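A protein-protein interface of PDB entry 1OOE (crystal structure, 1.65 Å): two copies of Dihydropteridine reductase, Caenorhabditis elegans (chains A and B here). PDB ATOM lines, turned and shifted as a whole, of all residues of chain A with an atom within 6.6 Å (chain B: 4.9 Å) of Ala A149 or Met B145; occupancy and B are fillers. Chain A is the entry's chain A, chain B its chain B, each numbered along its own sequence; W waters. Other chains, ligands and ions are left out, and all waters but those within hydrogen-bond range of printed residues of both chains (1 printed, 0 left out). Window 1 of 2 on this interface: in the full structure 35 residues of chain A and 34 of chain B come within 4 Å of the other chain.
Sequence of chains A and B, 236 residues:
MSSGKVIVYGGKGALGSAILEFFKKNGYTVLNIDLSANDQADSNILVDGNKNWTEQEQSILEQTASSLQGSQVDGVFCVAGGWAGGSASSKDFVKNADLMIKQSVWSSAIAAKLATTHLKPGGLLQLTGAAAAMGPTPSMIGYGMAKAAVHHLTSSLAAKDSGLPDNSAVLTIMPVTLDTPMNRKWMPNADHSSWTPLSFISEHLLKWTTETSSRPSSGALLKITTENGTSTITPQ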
ATOM      1  N   TRP A  53      25.589 -26.997  20.433  1.00  0.00           N
ATOM      2  CA  TRP A  53      26.691 -26.226  19.862  1.00  0.00           C
ATOM      3  C   TRP A  53      27.895 -26.071  20.788  1.00  0.00           C
ATOM      4  O   TRP A  53      29.016 -26.408  20.408  1.00  0.00           O
ATOM      5  CB  TRP A  53      26.193 -24.841  19.435  1.00  0.00           C
ATOM      6  CG  TRP A  53      27.006 -24.184  18.340  1.00  0.00           C
ATOM      7  CD1 TRP A  53      28.236 -24.567  17.870  1.00  0.00           C
ATOM      8  CD2 TRP A  53      26.643 -23.015  17.596  1.00  0.00           C
ATOM      9  NE1 TRP A  53      28.656 -23.704  16.879  1.00  0.00           N
ATOM     10  CE2 TRP A  53      27.696 -22.744  16.693  1.00  0.00           C
ATOM     11  CE3 TRP A  53      25.525 -22.170  17.606  1.00  0.00           C
ATOM     12  CZ2 TRP A  53      27.663 -21.659  15.808  1.00  0.00           C
ATOM     13  CZ3 TRP A  53      25.492 -21.098  16.729  1.00  0.00           C
ATOM     14  CH2 TRP A  53      26.555 -20.850  15.841  1.00  0.00           C
ATOM     15  N   ILE A 101      21.288 -24.742  10.042  1.00  0.00           N
ATOM     16  CA  ILE A 101      22.162 -23.946  10.899  1.00  0.00           C
ATOM     17  C   ILE A 101      23.158 -24.921  11.529  1.00  0.00           C
ATOM     18  O   ILE A 101      24.369 -24.675  11.545  1.00  0.00           O
ATOM     19  CB  ILE A 101      21.377 -23.240  12.031  1.00  0.00           C
ATOM     20  CG1 ILE A 101      20.481 -22.138  11.449  1.00  0.00           C
ATOM     21  CG2 ILE A 101      22.346 -22.676  13.073  1.00  0.00           C
ATOM     22  CD1 ILE A 101      21.220 -20.923  10.914  1.00  0.00           C
ATOM     23  N   VAL A 105      26.424 -23.644   9.787  1.00  0.00           N
ATOM     24  CA  VAL A 105      26.885 -22.614  10.710  1.00  0.00           C
ATOM     25  C   VAL A 105      27.674 -23.148  11.904  1.00  0.00           C
ATOM     26  O   VAL A 105      28.719 -22.601  12.247  1.00  0.00           O
ATOM     27  CB  VAL A 105      25.700 -21.756  11.215  1.00  0.00           C
ATOM     28  CG1 VAL A 105      26.195 -20.701  12.197  1.00  0.00           C
ATOM     29  CG2 VAL A 105      25.016 -21.081  10.032  1.00  0.00           C
ATOM     30  N   ALA A 109      31.715 -22.231  12.269  1.00  0.00           N
ATOM     31  CA  ALA A 109      32.129 -21.472  13.444  1.00  0.00           C
ATOM     32  C   ALA A 109      33.170 -22.216  14.271  1.00  0.00           C
ATOM     33  O   ALA A 109      34.123 -21.612  14.754  1.00  0.00           O
ATOM     34  CB  ALA A 109      30.923 -21.144  14.302  1.00  0.00           C
ATOM     35  N   GLY A 144      19.364 -21.073   2.563  1.00  0.00           N
ATOM     36  CA  GLY A 144      19.813 -19.741   2.193  1.00  0.00           C
ATOM     37  C   GLY A 144      20.299 -18.929   3.379  1.00  0.00           C
ATOM     38  O   GLY A 144      21.370 -18.322   3.310  1.00  0.00           O
ATOM     39  N   MET A 145      19.513 -18.915   4.456  1.00  0.00           N
ATOM     40  CA  MET A 145      19.847 -18.180   5.682  1.00  0.00           C
ATOM     41  C   MET A 145      21.155 -18.648   6.296  1.00  0.00           C
ATOM     42  O   MET A 145      22.014 -17.841   6.661  1.00  0.00           O
ATOM     43  CB  MET A 145      18.781 -18.386   6.756  1.00  0.00           C
ATOM     44  CG  MET A 145      17.445 -17.759   6.511  1.00  0.00           C
ATOM     45  SD  MET A 145      16.623 -17.669   8.102  1.00  0.00           S
ATOM     46  CE  MET A 145      16.124 -19.355   8.361  1.00  0.00           C
ATOM     47  N   ALA A 146      21.259 -19.963   6.455  1.00  0.00           N
ATOM     48  CA  ALA A 146      22.432 -20.588   7.050  1.00  0.00           C
ATOM     49  C   ALA A 146      23.690 -20.235   6.274  1.00  0.00           C
ATOM     50  O   ALA A 146      24.691 -19.814   6.858  1.00  0.00           O
ATOM     51  CB  ALA A 146      22.250 -22.107   7.091  1.00  0.00           C
ATOM     52  N   LYS A 147      23.639 -20.400   4.956  1.00  0.00           N
ATOM     53  CA  LYS A 147      24.802 -20.097   4.137  1.00  0.00           C
ATOM     54  C   LYS A 147      25.122 -18.602   4.098  1.00  0.00           C
ATOM     55  O   LYS A 147      26.289 -18.225   4.003  1.00  0.00           O
ATOM     56  CB  LYS A 147      24.612 -20.662   2.724  1.00  0.00           C
ATOM     57  CG  LYS A 147      24.669 -22.190   2.668  1.00  0.00           C
ATOM     58  CD  LYS A 147      26.078 -22.710   2.966  1.00  0.00           C
ATOM     59  CE  LYS A 147      26.185 -24.209   2.714  1.00  0.00           C
ATOM     60  NZ  LYS A 147      27.592 -24.699   2.872  1.00  0.00           N
ATOM     61  N   ALA A 148      24.106 -17.745   4.182  1.00  0.00           N
ATOM     62  CA  ALA A 148      24.356 -16.303   4.183  1.00  0.00           C
ATOM     63  C   ALA A 148      25.134 -15.958   5.450  1.00  0.00           C
ATOM     64  O   ALA A 148      25.987 -15.070   5.436  1.00  0.00           O
ATOM     65  CB  ALA A 148      23.038 -15.518   4.142  1.00  0.00           C
ATOM     66  N   ALA A 149      24.839 -16.658   6.543  1.00  0.00           N
ATOM     67  CA  ALA A 149      25.545 -16.410   7.795  1.00  0.00           C
ATOM     68  C   ALA A 149      27.011 -16.798   7.616  1.00  0.00           C
ATOM     69  O   ALA A 149      27.900 -16.098   8.104  1.00  0.00           O
ATOM     70  CB  ALA A 149      24.918 -17.209   8.939  1.00  0.00           C
ATOM     71  N   VAL A 150      27.266 -17.901   6.913  1.00  0.00           N
ATOM     72  CA  VAL A 150      28.644 -18.340   6.679  1.00  0.00           C
ATOM     73  C   VAL A 150      29.369 -17.300   5.822  1.00  0.00           C
ATOM     74  O   VAL A 150      30.542 -17.010   6.047  1.00  0.00           O
ATOM     75  CB  VAL A 150      28.700 -19.731   5.986  1.00  0.00           C
ATOM     76  CG1 VAL A 150      30.148 -20.081   5.613  1.00  0.00           C
ATOM     77  CG2 VAL A 150      28.147 -20.797   6.923  1.00  0.00           C
ATOM     78  N   HIS A 151      28.672 -16.734   4.841  1.00  0.00           N
ATOM     79  CA  HIS A 151      29.284 -15.712   3.997  1.00  0.00           C
ATOM     80  C   HIS A 151      29.641 -14.489   4.852  1.00  0.00           C
ATOM     81  O   HIS A 151      30.703 -13.893   4.671  1.00  0.00           O
ATOM     82  CB  HIS A 151      28.337 -15.295   2.866  1.00  0.00           C
ATOM     83  CG  HIS A 151      28.122 -16.356   1.829  1.00  0.00           C
ATOM     84  ND1 HIS A 151      27.385 -16.136   0.684  1.00  0.00           N
ATOM     85  CD2 HIS A 151      28.540 -17.642   1.766  1.00  0.00           C
ATOM     86  CE1 HIS A 151      27.359 -17.241  -0.040  1.00  0.00           C
ATOM     87  NE2 HIS A 151      28.053 -18.172   0.594  1.00  0.00           N
ATOM     88  N   HIS A 152      28.769 -14.117   5.786  1.00  0.00           N
ATOM     89  CA  HIS A 152      29.060 -12.961   6.629  1.00  0.00           C
ATOM     90  C   HIS A 152      30.225 -13.263   7.570  1.00  0.00           C
ATOM     91  O   HIS A 152      31.095 -12.412   7.790  1.00  0.00           O
ATOM     92  CB  HIS A 152      27.835 -12.529   7.442  1.00  0.00           C
ATOM     93  CG  HIS A 152      28.030 -11.218   8.135  1.00  0.00           C
ATOM     94  ND1 HIS A 152      28.585 -11.115   9.393  1.00  0.00           N
ATOM     95  CD2 HIS A 152      27.868  -9.949   7.690  1.00  0.00           C
ATOM     96  CE1 HIS A 152      28.763  -9.839   9.689  1.00  0.00           C
ATOM     97  NE2 HIS A 152      28.339  -9.111   8.672  1.00  0.00           N
ATOM     98  N   LEU A 153      30.238 -14.480   8.108  1.00  0.00           N
ATOM     99  CA  LEU A 153      31.298 -14.921   9.011  1.00  0.00           C
ATOM    100  C   LEU A 153      32.632 -14.760   8.299  1.00  0.00           C
ATOM    101  O   LEU A 153      33.626 -14.329   8.887  1.00  0.00           O
ATOM    102  CB  LEU A 153      31.083 -16.391   9.387  1.00  0.00           C
ATOM    103  CG  LEU A 153      32.238 -17.132  10.074  1.00  0.00           C
ATOM    104  CD1 LEU A 153      32.584 -16.469  11.392  1.00  0.00           C
ATOM    105  CD2 LEU A 153      31.845 -18.574  10.303  1.00  0.00           C
ATOM    106  N   THR A 154      32.643 -15.116   7.020  1.00  0.00           N
ATOM    107  CA  THR A 154      33.844 -15.000   6.208  1.00  0.00           C
ATOM    108  C   THR A 154      34.357 -13.562   6.187  1.00  0.00           C
ATOM    109  O   THR A 154      35.559 -13.318   6.356  1.00  0.00           O
ATOM    110  CB  THR A 154      33.558 -15.474   4.771  1.00  0.00           C
ATOM    111  OG1 THR A 154      33.209 -16.863   4.804  1.00  0.00           O
ATOM    112  CG2 THR A 154      34.783 -15.285   3.882  1.00  0.00           C
ATOM    113  N   SER A 156      33.773 -11.167   8.389  1.00  0.00           N
ATOM    114  CA  SER A 156      34.223 -10.757   9.719  1.00  0.00           C
ATOM    115  C   SER A 156      35.602 -11.330  10.054  1.00  0.00           C
ATOM    116  O   SER A 156      36.437 -10.646  10.639  1.00  0.00           O
ATOM    117  CB  SER A 156      33.214 -11.192  10.784  1.00  0.00           C
ATOM    118  OG  SER A 156      31.994 -10.482  10.645  1.00  0.00           O
ATOM    119  N   ALA B  97      27.386 -16.825  19.841  1.00  0.00           N
ATOM    120  CA  ALA B  97      26.850 -17.027  18.499  1.00  0.00           C
ATOM    121  C   ALA B  97      25.554 -17.823  18.652  1.00  0.00           C
ATOM    122  O   ALA B  97      24.556 -17.562  17.973  1.00  0.00           O
ATOM    123  CB  ALA B  97      27.844 -17.805  17.639  1.00  0.00           C
ATOM    124  N   ILE B 101      21.809 -16.504  17.470  1.00  0.00           N
ATOM    125  CA  ILE B 101      20.988 -17.198  16.478  1.00  0.00           C
ATOM    126  C   ILE B 101      19.593 -17.438  17.071  1.00  0.00           C
ATOM    127  O   ILE B 101      18.572 -17.222  16.410  1.00  0.00           O
ATOM    128  CB  ILE B 101      21.619 -18.554  16.062  1.00  0.00           C
ATOM    129  CG1 ILE B 101      22.877 -18.309  15.216  1.00  0.00           C
ATOM    130  CG2 ILE B 101      20.603 -19.397  15.296  1.00  0.00           C
ATOM    131  CD1 ILE B 101      22.617 -17.630  13.892  1.00  0.00           C
ATOM    132  N   ILE B 141      31.206 -11.159  16.048  1.00  0.00           N
ATOM    133  CA  ILE B 141      30.970 -12.089  14.954  1.00  0.00           C
ATOM    134  C   ILE B 141      29.645 -12.851  14.994  1.00  0.00           C
ATOM    135  O   ILE B 141      28.968 -12.964  13.967  1.00  0.00           O
ATOM    136  CB  ILE B 141      32.158 -13.066  14.841  1.00  0.00           C
ATOM    137  CG1 ILE B 141      33.439 -12.266  14.563  1.00  0.00           C
ATOM    138  CG2 ILE B 141      31.927 -14.053  13.704  1.00  0.00           C
ATOM    139  CD1 ILE B 141      34.687 -13.108  14.404  1.00  0.00           C
ATOM    140  N   GLY B 142      29.267 -13.362  16.162  1.00  0.00           N
ATOM    141  CA  GLY B 142      28.011 -14.094  16.263  1.00  0.00           C
ATOM    142  C   GLY B 142      26.804 -13.225  15.950  1.00  0.00           C
ATOM    143  O   GLY B 142      25.878 -13.645  15.246  1.00  0.00           O
ATOM    144  N   TYR B 143      26.802 -12.008  16.485  1.00  0.00           N
ATOM    145  CA  TYR B 143      25.708 -11.073  16.248  1.00  0.00           C
ATOM    146  C   TYR B 143      25.614 -10.769  14.754  1.00  0.00           C
ATOM    147  O   TYR B 143      24.523 -10.756  14.178  1.00  0.00           O
ATOM    148  CB  TYR B 143      25.958  -9.777  17.020  1.00  0.00           C
ATOM    149  CG  TYR B 143      24.879  -8.728  16.869  1.00  0.00           C
ATOM    150  CD1 TYR B 143      23.629  -8.887  17.467  1.00  0.00           C
ATOM    151  CD2 TYR B 143      25.123  -7.552  16.158  1.00  0.00           C
ATOM    152  CE1 TYR B 143      22.648  -7.896  17.363  1.00  0.00           C
ATOM    153  CE2 TYR B 143      24.152  -6.558  16.049  1.00  0.00           C
ATOM    154  CZ  TYR B 143      22.917  -6.737  16.656  1.00  0.00           C
ATOM    155  OH  TYR B 143      21.959  -5.754  16.558  1.00  0.00           O
ATOM    156  N   GLY B 144      26.770 -10.536  14.138  1.00  0.00           N
ATOM    157  CA  GLY B 144      26.822 -10.235  12.720  1.00  0.00           C
ATOM    158  C   GLY B 144      26.263 -11.358  11.867  1.00  0.00           C
ATOM    159  O   GLY B 144      25.505 -11.097  10.933  1.00  0.00           O
ATOM    160  N   MET B 145      26.638 -12.598  12.184  1.00  0.00           N
ATOM    161  CA  MET B 145      26.174 -13.781  11.444  1.00  0.00           C
ATOM    162  C   MET B 145      24.665 -13.921  11.511  1.00  0.00           C
ATOM    163  O   MET B 145      23.998 -14.133  10.496  1.00  0.00           O
ATOM    164  CB  MET B 145      26.737 -15.069  12.039  1.00  0.00           C
ATOM    165  CG  MET B 145      28.214 -15.248  11.971  1.00  0.00           C
ATOM    166  SD  MET B 145      28.542 -16.989  12.256  1.00  0.00           S
ATOM    167  CE  MET B 145      28.055 -17.194  13.970  1.00  0.00           C
ATOM    168  N   ALA B 146      24.148 -13.852  12.733  1.00  0.00           N
ATOM    169  CA  ALA B 146      22.720 -13.987  12.981  1.00  0.00           C
ATOM    170  C   ALA B 146      21.924 -12.926  12.240  1.00  0.00           C
ATOM    171  O   ALA B 146      20.940 -13.233  11.562  1.00  0.00           O
ATOM    172  CB  ALA B 146      22.440 -13.906  14.480  1.00  0.00           C
ATOM    173  N   LYS B 147      22.343 -11.672  12.366  1.00  0.00           N
ATOM    174  CA  LYS B 147      21.631 -10.603  11.686  1.00  0.00           C
ATOM    175  C   LYS B 147      21.743 -10.705  10.165  1.00  0.00           C
ATOM    176  O   LYS B 147      20.793 -10.372   9.458  1.00  0.00           O
ATOM    177  CB  LYS B 147      22.112  -9.242  12.192  1.00  0.00           C
ATOM    178  CG  LYS B 147      21.638  -8.920  13.615  1.00  0.00           C
ATOM    179  CD  LYS B 147      20.114  -8.795  13.689  1.00  0.00           C
ATOM    180  CE  LYS B 147      19.657  -8.325  15.068  1.00  0.00           C
ATOM    181  NZ  LYS B 147      18.222  -7.909  15.054  1.00  0.00           N
ATOM    182  N   ALA B 148      22.881 -11.178   9.657  1.00  0.00           N
ATOM    183  CA  ALA B 148      23.036 -11.324   8.208  1.00  0.00           C
ATOM    184  C   ALA B 148      22.044 -12.367   7.702  1.00  0.00           C
ATOM    185  O   ALA B 148      21.528 -12.259   6.591  1.00  0.00           O
ATOM    186  CB  ALA B 148      24.466 -11.738   7.855  1.00  0.00           C
ATOM    187  N   ALA B 149      21.776 -13.375   8.527  1.00  0.00           N
ATOM    188  CA  ALA B 149      20.829 -14.421   8.154  1.00  0.00           C
ATOM    189  C   ALA B 149      19.429 -13.819   8.058  1.00  0.00           C
ATOM    190  O   ALA B 149      18.658 -14.181   7.170  1.00  0.00           O
ATOM    191  CB  ALA B 149      20.853 -15.545   9.180  1.00  0.00           C
HETATM  192  O   HOH W   1      30.146 -12.369  11.268  1.00  0.00           O
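Hydrophobic or aromatic side chains of chain B within 4 Å of the printed part of chain A: Ala B97, Ile B141, Met B145, Ala B148 and Ala B149. Along chain B the printed residues that touch a printed residue of chain A span positions 97 to 149. Of the 16 printed residues of chain A, 6 touch a printed residue of chain B. Printed residues of chain A that touch a printed residue of chain B: Trp A53, Met A145, Ala A149, His A152, Leu A153 and Ser A156. Hydrophobic or aromatic side chains of chain A within 4 Å of the printed part of chain B: Trp A53, Met A145, Ala A149, His A152 and Leu A153. Among the printed residues, 9 pairs touch across the chains. Among the printed residues, no Asp or Glu carboxylate lies within 4 Å of a Lys or Arg side-chain nitrogen of the other chain.
Of chain B, only Met B145 comes within 4 Å of Ala A149. Met B145 touches just these residues of chain A: Ala A149, His A152 and Leu A153. Of the printed residues of chain A, Ala B149 touches Met A145. Of the printed residues of chain B, His A152 touches Gly B144, Met B145 and Ala B148. Printed residues of chain A within 4 Å of Gly B144: His A152. Printed residues of chain A within 4 Å of Ala B97: Trp A53 (3.8 Å). The nearest printed residue of chain B that does not touch Met A145 is Ala B148 (5.6 Å).
Met A145 touches Ala B149, and with the chains exchanged Ala A149 touches Met B145. Positions printed for both chains: 101, 144, 145, 146, 147, 148 and 149.
A ring nitrogen (ND1) of His A152 sits close to the backbone carbonyl oxygen (O) of Gly B144 (3.4 Å).
CH2 of Trp A53 touches CB of Ala B97, 3.8 Å away. O of Met A145 touches CB of Ala B149 (3.6 Å). O of Met B145 touches CB of Ala A149, 3.6 Å away. His A152 touches Met B145 (ND1 to N, 3.7 Å). His A152 touches Ala B148. CD1 of Leu A153 touches CG2 of Ile B141, 3.4 Å away. CB of Leu A153 touches SD of Met B145, at 3.9 Å. Ser A156 touches Ile B141 (CB to CG1, 3.9 Å).
Water W1 lies within hydrogen-bond range of OG of Ser A156 (2.7 Å), ND1 of His A152 (2.7 Å) and O of Ile B141 (3.0 Å).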
